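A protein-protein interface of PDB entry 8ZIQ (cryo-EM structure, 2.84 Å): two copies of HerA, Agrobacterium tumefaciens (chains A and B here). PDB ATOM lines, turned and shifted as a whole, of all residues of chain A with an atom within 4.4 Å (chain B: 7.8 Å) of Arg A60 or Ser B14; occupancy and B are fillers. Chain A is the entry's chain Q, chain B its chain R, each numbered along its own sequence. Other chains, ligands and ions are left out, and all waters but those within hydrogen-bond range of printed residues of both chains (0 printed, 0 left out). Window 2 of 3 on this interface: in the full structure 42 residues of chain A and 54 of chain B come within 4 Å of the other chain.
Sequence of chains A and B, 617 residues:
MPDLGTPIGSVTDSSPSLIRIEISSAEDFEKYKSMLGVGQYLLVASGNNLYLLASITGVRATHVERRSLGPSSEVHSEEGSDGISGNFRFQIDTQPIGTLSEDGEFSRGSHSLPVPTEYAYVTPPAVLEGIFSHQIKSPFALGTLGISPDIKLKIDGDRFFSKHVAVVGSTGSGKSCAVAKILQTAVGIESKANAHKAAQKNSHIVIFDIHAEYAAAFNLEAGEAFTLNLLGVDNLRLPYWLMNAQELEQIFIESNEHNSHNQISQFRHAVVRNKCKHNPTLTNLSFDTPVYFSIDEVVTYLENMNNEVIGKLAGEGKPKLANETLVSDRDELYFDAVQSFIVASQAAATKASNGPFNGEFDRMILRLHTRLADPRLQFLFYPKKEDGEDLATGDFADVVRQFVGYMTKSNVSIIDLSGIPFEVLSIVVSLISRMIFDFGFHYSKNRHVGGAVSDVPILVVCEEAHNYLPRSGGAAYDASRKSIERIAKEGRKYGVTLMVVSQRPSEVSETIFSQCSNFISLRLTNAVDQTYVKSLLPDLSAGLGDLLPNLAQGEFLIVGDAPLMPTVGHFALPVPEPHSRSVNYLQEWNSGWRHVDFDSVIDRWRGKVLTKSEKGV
No position is printed for both chains.
Of the 7 pairs that touch across the chains among the printed residues, none has its exchanged pair printed and touching as well.
Printed residues of chain B that touch a printed residue of chain A: Asp B13, Ser B14, Ser B15, Pro B16 and Leu B113.
Hydrophobic or aromatic side chains of chain B within 4 Å of the printed part of chain A: Pro B16 and Leu B113.
Hydrophobic or aromatic side chains of chain A within 4 Å of the printed part of chain B: Val A59.
Of the printed residues of chain B, Arg A60 touches Ser B14.
Ala A61 touches just these residues of chain B: Asp B13 (3.8 Å) and Ser B14 (3.4 Å).
Printed residues of chain B within 4 Å of Thr A62: Asp B13.
Of the printed residues of chain A, Ser B14 touches Arg A60 (3.997 Å) and Ala A61 (3.4 Å).
Of the printed residues of chain A, Ser B15 touches Val A59.
Leu B18 touches none of the printed residues of chain A.
O of Val A59 touches OG of Ser B15 (3.7 Å).
Pro B16 touches Val A59 (CD to O, 3.6 Å).
Leu B113 touches Val A59.
Ser B14 touches Arg A60 (O to CA, 3.997 Å).
CA of Asp B13 touches O of Ala A61, at 3.8 Å.
Thr A62 touches Asp B13.
The backbone NH (N) of Arg A89 sits at hydrogen-bond distance from the backbone carbonyl oxygen (O) of Thr A62 (2.9 Å).
O of Arg A60 sits at hydrogen-bond distance from N of Gln A91 (2.9 Å).
OD2 of Asp B13 lies within salt-bridge range of NH1 of Arg B20.
The side-chain hydroxyl of Ser B14 is in hydrogen-bond range of the backbone carbonyl oxygen of Pro B114.
The side-chain hydroxyl of Thr B12 is in hydrogen-bond range of the side-chain carboxylate of Asp B13 (3.3 Å).
The backbone NH (N) of Ser B14 sits at hydrogen-bond distance from the backbone carbonyl oxygen (O) of Ala A61 (3.4 Å).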
ATOM      1  N   VAL A  59      -1.265  -0.589 -14.988  1.00  0.00           N
ATOM      2  CA  VAL A  59      -0.054   0.197 -14.798  1.00  0.00           C
ATOM      3  C   VAL A  59       0.234   0.272 -13.309  1.00  0.00           C
ATOM      4  O   VAL A  59      -0.656   0.593 -12.516  1.00  0.00           O
ATOM      5  CB  VAL A  59      -0.182   1.616 -15.370  1.00  0.00           C
ATOM      6  CG1 VAL A  59       1.077   2.368 -15.158  1.00  0.00           C
ATOM      7  CG2 VAL A  59      -0.499   1.584 -16.810  1.00  0.00           C
ATOM      8  N   ARG A  60       1.471  -0.018 -12.929  1.00  0.00           N
ATOM      9  CA  ARG A  60       1.914   0.058 -11.546  1.00  0.00           C
ATOM     10  C   ARG A  60       3.224   0.820 -11.470  1.00  0.00           C
ATOM     11  O   ARG A  60       4.075   0.687 -12.351  1.00  0.00           O
ATOM     12  CB  ARG A  60       2.086  -1.314 -10.927  1.00  0.00           C
ATOM     13  CG  ARG A  60       0.813  -2.089 -10.760  1.00  0.00           C
ATOM     14  CD  ARG A  60       1.090  -3.461 -10.172  1.00  0.00           C
ATOM     15  NE  ARG A  60      -0.110  -4.291 -10.097  1.00  0.00           N
ATOM     16  CZ  ARG A  60      -0.110  -5.574  -9.750  1.00  0.00           C
ATOM     17  NH1 ARG A  60       1.028  -6.188  -9.454  1.00  0.00           N
ATOM     18  NH2 ARG A  60      -1.249  -6.252  -9.708  1.00  0.00           N
ATOM     19  N   ALA A  61       3.384   1.626 -10.425  1.00  0.00           N
ATOM     20  CA  ALA A  61       4.563   2.467 -10.268  1.00  0.00           C
ATOM     21  C   ALA A  61       5.038   2.404  -8.832  1.00  0.00           C
ATOM     22  O   ALA A  61       4.270   2.686  -7.910  1.00  0.00           O
ATOM     23  CB  ALA A  61       4.275   3.908 -10.660  1.00  0.00           C
ATOM     24  N   THR A  62       6.300   2.030  -8.643  1.00  0.00           N
ATOM     25  CA  THR A  62       6.859   1.874  -7.312  1.00  0.00           C
ATOM     26  C   THR A  62       8.313   2.314  -7.285  1.00  0.00           C
ATOM     27  O   THR A  62       9.078   2.035  -8.212  1.00  0.00           O
ATOM     28  CB  THR A  62       6.765   0.428  -6.839  1.00  0.00           C
ATOM     29  OG1 THR A  62       7.345  -0.437  -7.821  1.00  0.00           O
ATOM     30  CG2 THR A  62       5.319   0.032  -6.610  1.00  0.00           C
ATOM     31  N   ARG A  89      10.493   1.850 -10.715  1.00  0.00           N
ATOM     32  CA  ARG A  89       9.915   0.741 -11.454  1.00  0.00           C
ATOM     33  C   ARG A  89       8.536   1.106 -11.974  1.00  0.00           C
ATOM     34  O   ARG A  89       7.688   1.565 -11.205  1.00  0.00           O
ATOM     35  CB  ARG A  89       9.730  -0.507 -10.596  1.00  0.00           C
ATOM     36  CG  ARG A  89       9.980  -1.799 -11.322  1.00  0.00           C
ATOM     37  CD  ARG A  89      10.002  -2.974 -10.368  1.00  0.00           C
ATOM     38  NE  ARG A  89       9.689  -4.215 -11.071  1.00  0.00           N
ATOM     39  CZ  ARG A  89       9.837  -5.435 -10.564  1.00  0.00           C
ATOM     40  NH1 ARG A  89      10.308  -5.610  -9.336  1.00  0.00           N
ATOM     41  NH2 ARG A  89       9.505  -6.487 -11.297  1.00  0.00           N
ATOM     42  N   PHE A  90       8.310   0.888 -13.266  1.00  0.00           N
ATOM     43  CA  PHE A  90       7.006   1.083 -13.877  1.00  0.00           C
ATOM     44  C   PHE A  90       6.668  -0.180 -14.647  1.00  0.00           C
ATOM     45  O   PHE A  90       7.422  -0.581 -15.535  1.00  0.00           O
ATOM     46  CB  PHE A  90       6.990   2.300 -14.797  1.00  0.00           C
ATOM     47  CG  PHE A  90       7.318   3.584 -14.121  1.00  0.00           C
ATOM     48  CD1 PHE A  90       6.358   4.260 -13.402  1.00  0.00           C
ATOM     49  CD2 PHE A  90       8.579   4.108 -14.179  1.00  0.00           C
ATOM     50  CE1 PHE A  90       6.655   5.441 -12.789  1.00  0.00           C
ATOM     51  CE2 PHE A  90       8.867   5.284 -13.561  1.00  0.00           C
ATOM     52  CZ  PHE A  90       7.913   5.939 -12.857  1.00  0.00           C
ATOM     53  N   GLN A  91       5.537  -0.793 -14.322  1.00  0.00           N
ATOM     54  CA  GLN A  91       5.089  -2.020 -14.957  1.00  0.00           C
ATOM     55  C   GLN A  91       3.826  -1.761 -15.758  1.00  0.00           C
ATOM     56  O   GLN A  91       2.909  -1.080 -15.285  1.00  0.00           O
ATOM     57  CB  GLN A  91       4.812  -3.128 -13.945  1.00  0.00           C
ATOM     58  CG  GLN A  91       5.947  -3.499 -13.042  1.00  0.00           C
ATOM     59  CD  GLN A  91       5.775  -4.888 -12.474  1.00  0.00           C
ATOM     60  OE1 GLN A  91       4.700  -5.247 -11.999  1.00  0.00           O
ATOM     61  NE2 GLN A  91       6.835  -5.685 -12.528  1.00  0.00           N
ATOM     62  N   VAL B  11       4.232  10.117  -1.659  1.00  0.00           N
ATOM     63  CA  VAL B  11       3.635   8.953  -2.291  1.00  0.00           C
ATOM     64  C   VAL B  11       4.652   7.829  -2.369  1.00  0.00           C
ATOM     65  O   VAL B  11       5.835   8.053  -2.645  1.00  0.00           O
ATOM     66  CB  VAL B  11       3.126   9.332  -3.688  1.00  0.00           C
ATOM     67  CG1 VAL B  11       2.745   8.126  -4.459  1.00  0.00           C
ATOM     68  CG2 VAL B  11       1.980  10.272  -3.587  1.00  0.00           C
ATOM     69  N   THR B  12       4.184   6.603  -2.131  1.00  0.00           N
ATOM     70  CA  THR B  12       5.006   5.413  -2.249  1.00  0.00           C
ATOM     71  C   THR B  12       4.501   4.398  -3.257  1.00  0.00           C
ATOM     72  O   THR B  12       5.309   3.623  -3.775  1.00  0.00           O
ATOM     73  CB  THR B  12       5.132   4.715  -0.888  1.00  0.00           C
ATOM     74  OG1 THR B  12       3.968   3.925  -0.638  1.00  0.00           O
ATOM     75  CG2 THR B  12       5.285   5.723   0.212  1.00  0.00           C
ATOM     76  N   ASP B  13       3.207   4.373  -3.553  1.00  0.00           N
ATOM     77  CA  ASP B  13       2.664   3.446  -4.532  1.00  0.00           C
ATOM     78  C   ASP B  13       1.498   4.105  -5.248  1.00  0.00           C
ATOM     79  O   ASP B  13       0.640   4.733  -4.617  1.00  0.00           O
ATOM     80  CB  ASP B  13       2.216   2.136  -3.883  1.00  0.00           C
ATOM     81  CG  ASP B  13       3.354   1.399  -3.197  1.00  0.00           C
ATOM     82  OD1 ASP B  13       4.408   1.188  -3.832  1.00  0.00           O
ATOM     83  OD2 ASP B  13       3.193   1.028  -2.015  1.00  0.00           O
ATOM     84  N   SER B  14       1.470   3.945  -6.563  1.00  0.00           N
ATOM     85  CA  SER B  14       0.497   4.600  -7.415  1.00  0.00           C
ATOM     86  C   SER B  14      -0.100   3.609  -8.398  1.00  0.00           C
ATOM     87  O   SER B  14       0.553   2.661  -8.836  1.00  0.00           O
ATOM     88  CB  SER B  14       1.104   5.753  -8.177  1.00  0.00           C
ATOM     89  OG  SER B  14       0.212   6.238  -9.159  1.00  0.00           O
ATOM     90  N   SER B  15      -1.358   3.849  -8.734  1.00  0.00           N
ATOM     91  CA  SER B  15      -2.100   3.062  -9.704  1.00  0.00           C
ATOM     92  C   SER B  15      -3.372   3.822 -10.042  1.00  0.00           C
ATOM     93  O   SER B  15      -3.789   4.699  -9.282  1.00  0.00           O
ATOM     94  CB  SER B  15      -2.429   1.666  -9.165  1.00  0.00           C
ATOM     95  OG  SER B  15      -1.251   0.941  -8.873  1.00  0.00           O
ATOM     96  N   PRO B  16      -3.998   3.514 -11.177  1.00  0.00           N
ATOM     97  CA  PRO B  16      -5.206   4.254 -11.557  1.00  0.00           C
ATOM     98  C   PRO B  16      -6.284   4.221 -10.500  1.00  0.00           C
ATOM     99  O   PRO B  16      -7.039   5.188 -10.362  1.00  0.00           O
ATOM    100  CB  PRO B  16      -5.650   3.538 -12.831  1.00  0.00           C
ATOM    101  CG  PRO B  16      -4.429   2.998 -13.383  1.00  0.00           C
ATOM    102  CD  PRO B  16      -3.588   2.582 -12.232  1.00  0.00           C
ATOM    103  N   SER B  17      -6.394   3.124  -9.764  1.00  0.00           N
ATOM    104  CA  SER B  17      -7.416   2.994  -8.744  1.00  0.00           C
ATOM    105  C   SER B  17      -6.961   3.474  -7.373  1.00  0.00           C
ATOM    106  O   SER B  17      -7.708   4.186  -6.694  1.00  0.00           O
ATOM    107  CB  SER B  17      -7.866   1.540  -8.659  1.00  0.00           C
ATOM    108  OG  SER B  17      -8.462   1.257  -7.406  1.00  0.00           O
ATOM    109  N   LEU B  18      -5.757   3.103  -6.941  1.00  0.00           N
ATOM    110  CA  LEU B  18      -5.349   3.270  -5.555  1.00  0.00           C
ATOM    111  C   LEU B  18      -4.038   4.028  -5.447  1.00  0.00           C
ATOM    112  O   LEU B  18      -3.075   3.709  -6.148  1.00  0.00           O
ATOM    113  CB  LEU B  18      -5.200   1.916  -4.873  1.00  0.00           C
ATOM    114  CG  LEU B  18      -4.924   1.915  -3.379  1.00  0.00           C
ATOM    115  CD1 LEU B  18      -6.101   2.496  -2.624  1.00  0.00           C
ATOM    116  CD2 LEU B  18      -4.634   0.521  -2.919  1.00  0.00           C
ATOM    117  N   ILE B  19      -4.011   5.031  -4.577  1.00  0.00           N
ATOM    118  CA  ILE B  19      -2.801   5.766  -4.236  1.00  0.00           C
ATOM    119  C   ILE B  19      -2.496   5.521  -2.768  1.00  0.00           C
ATOM    120  O   ILE B  19      -3.404   5.359  -1.948  1.00  0.00           O
ATOM    121  CB  ILE B  19      -2.900   7.275  -4.524  1.00  0.00           C
ATOM    122  CG1 ILE B  19      -3.272   7.529  -5.967  1.00  0.00           C
ATOM    123  CG2 ILE B  19      -1.595   7.947  -4.262  1.00  0.00           C
ATOM    124  CD1 ILE B  19      -3.925   8.829  -6.169  1.00  0.00           C
ATOM    125  N   ARG B  20      -1.211   5.473  -2.438  1.00  0.00           N
ATOM    126  CA  ARG B  20      -0.765   5.148  -1.094  1.00  0.00           C
ATOM    127  C   ARG B  20       0.280   6.166  -0.663  1.00  0.00           C
ATOM    128  O   ARG B  20       1.258   6.398  -1.378  1.00  0.00           O
ATOM    129  CB  ARG B  20      -0.217   3.728  -1.047  1.00  0.00           C
ATOM    130  CG  ARG B  20       0.482   3.336   0.221  1.00  0.00           C
ATOM    131  CD  ARG B  20       0.799   1.856   0.205  1.00  0.00           C
ATOM    132  NE  ARG B  20      -0.409   1.047   0.293  1.00  0.00           N
ATOM    133  CZ  ARG B  20      -0.564  -0.151  -0.263  1.00  0.00           C
ATOM    134  NH1 ARG B  20       0.408  -0.700  -0.977  1.00  0.00           N
ATOM    135  NH2 ARG B  20      -1.709  -0.798  -0.115  1.00  0.00           N
ATOM    136  N   ILE B  21       0.068   6.767   0.506  1.00  0.00           N
ATOM    137  CA  ILE B  21       0.961   7.766   1.076  1.00  0.00           C
ATOM    138  C   ILE B  21       1.513   7.240   2.390  1.00  0.00           C
ATOM    139  O   ILE B  21       0.871   6.441   3.085  1.00  0.00           O
ATOM    140  CB  ILE B  21       0.249   9.120   1.291  1.00  0.00           C
ATOM    141  CG1 ILE B  21      -0.572   9.509   0.068  1.00  0.00           C
ATOM    142  CG2 ILE B  21       1.230  10.209   1.648  1.00  0.00           C
ATOM    143  CD1 ILE B  21      -1.475  10.641   0.307  1.00  0.00           C
ATOM    144  N   SER B 112      -4.472  10.925 -15.153  1.00  0.00           N
ATOM    145  CA  SER B 112      -3.072  11.037 -14.782  1.00  0.00           C
ATOM    146  C   SER B 112      -2.646   9.853 -13.921  1.00  0.00           C
ATOM    147  O   SER B 112      -3.404   8.909 -13.682  1.00  0.00           O
ATOM    148  CB  SER B 112      -2.820  12.366 -14.080  1.00  0.00           C
ATOM    149  OG  SER B 112      -3.248  13.447 -14.890  1.00  0.00           O
ATOM    150  N   LEU B 113      -1.406   9.898 -13.464  1.00  0.00           N
ATOM    151  CA  LEU B 113      -0.847   8.859 -12.621  1.00  0.00           C
ATOM    152  C   LEU B 113       0.338   9.441 -11.863  1.00  0.00           C
ATOM    153  O   LEU B 113       1.466   9.450 -12.371  1.00  0.00           O
ATOM    154  CB  LEU B 113      -0.427   7.661 -13.468  1.00  0.00           C
ATOM    155  CG  LEU B 113       0.010   6.379 -12.769  1.00  0.00           C
ATOM    156  CD1 LEU B 113      -0.301   5.172 -13.630  1.00  0.00           C
ATOM    157  CD2 LEU B 113       1.472   6.405 -12.441  1.00  0.00           C
ATOM    158  N   PRO B 114       0.114   9.943 -10.651  1.00  0.00           N
ATOM    159  CA  PRO B 114       1.172  10.660  -9.938  1.00  0.00           C
ATOM    160  C   PRO B 114       2.354   9.763  -9.625  1.00  0.00           C
ATOM    161  O   PRO B 114       2.197   8.602  -9.247  1.00  0.00           O
ATOM    162  CB  PRO B 114       0.475  11.132  -8.662  1.00  0.00           C
ATOM    163  CG  PRO B 114      -0.717  10.350  -8.560  1.00  0.00           C
ATOM    164  CD  PRO B 114      -1.156  10.025  -9.924  1.00  0.00           C
ATOM    165  N   VAL B 115       3.549  10.321  -9.779  1.00  0.00           N
ATOM    166  CA  VAL B 115       4.779   9.558  -9.636  1.00  0.00           C
ATOM    167  C   VAL B 115       5.191   9.514  -8.173  1.00  0.00           C
ATOM    168  O   VAL B 115       4.887  10.439  -7.409  1.00  0.00           O
ATOM    169  CB  VAL B 115       5.916  10.145 -10.482  1.00  0.00           C
ATOM    170  CG1 VAL B 115       5.564  10.120 -11.911  1.00  0.00           C
ATOM    171  CG2 VAL B 115       6.258  11.561 -10.029  1.00  0.00           C
ATOM    172  N   PRO B 116       5.879   8.464  -7.749  1.00  0.00           N
ATOM    173  CA  PRO B 116       6.397   8.422  -6.388  1.00  0.00           C
ATOM    174  C   PRO B 116       7.384   9.543  -6.132  1.00  0.00           C
ATOM    175  O   PRO B 116       7.985  10.109  -7.047  1.00  0.00           O
ATOM    176  CB  PRO B 116       7.058   7.050  -6.315  1.00  0.00           C
ATOM    177  CG  PRO B 116       6.336   6.272  -7.284  1.00  0.00           C
ATOM    178  CD  PRO B 116       6.004   7.159  -8.398  1.00  0.00           C
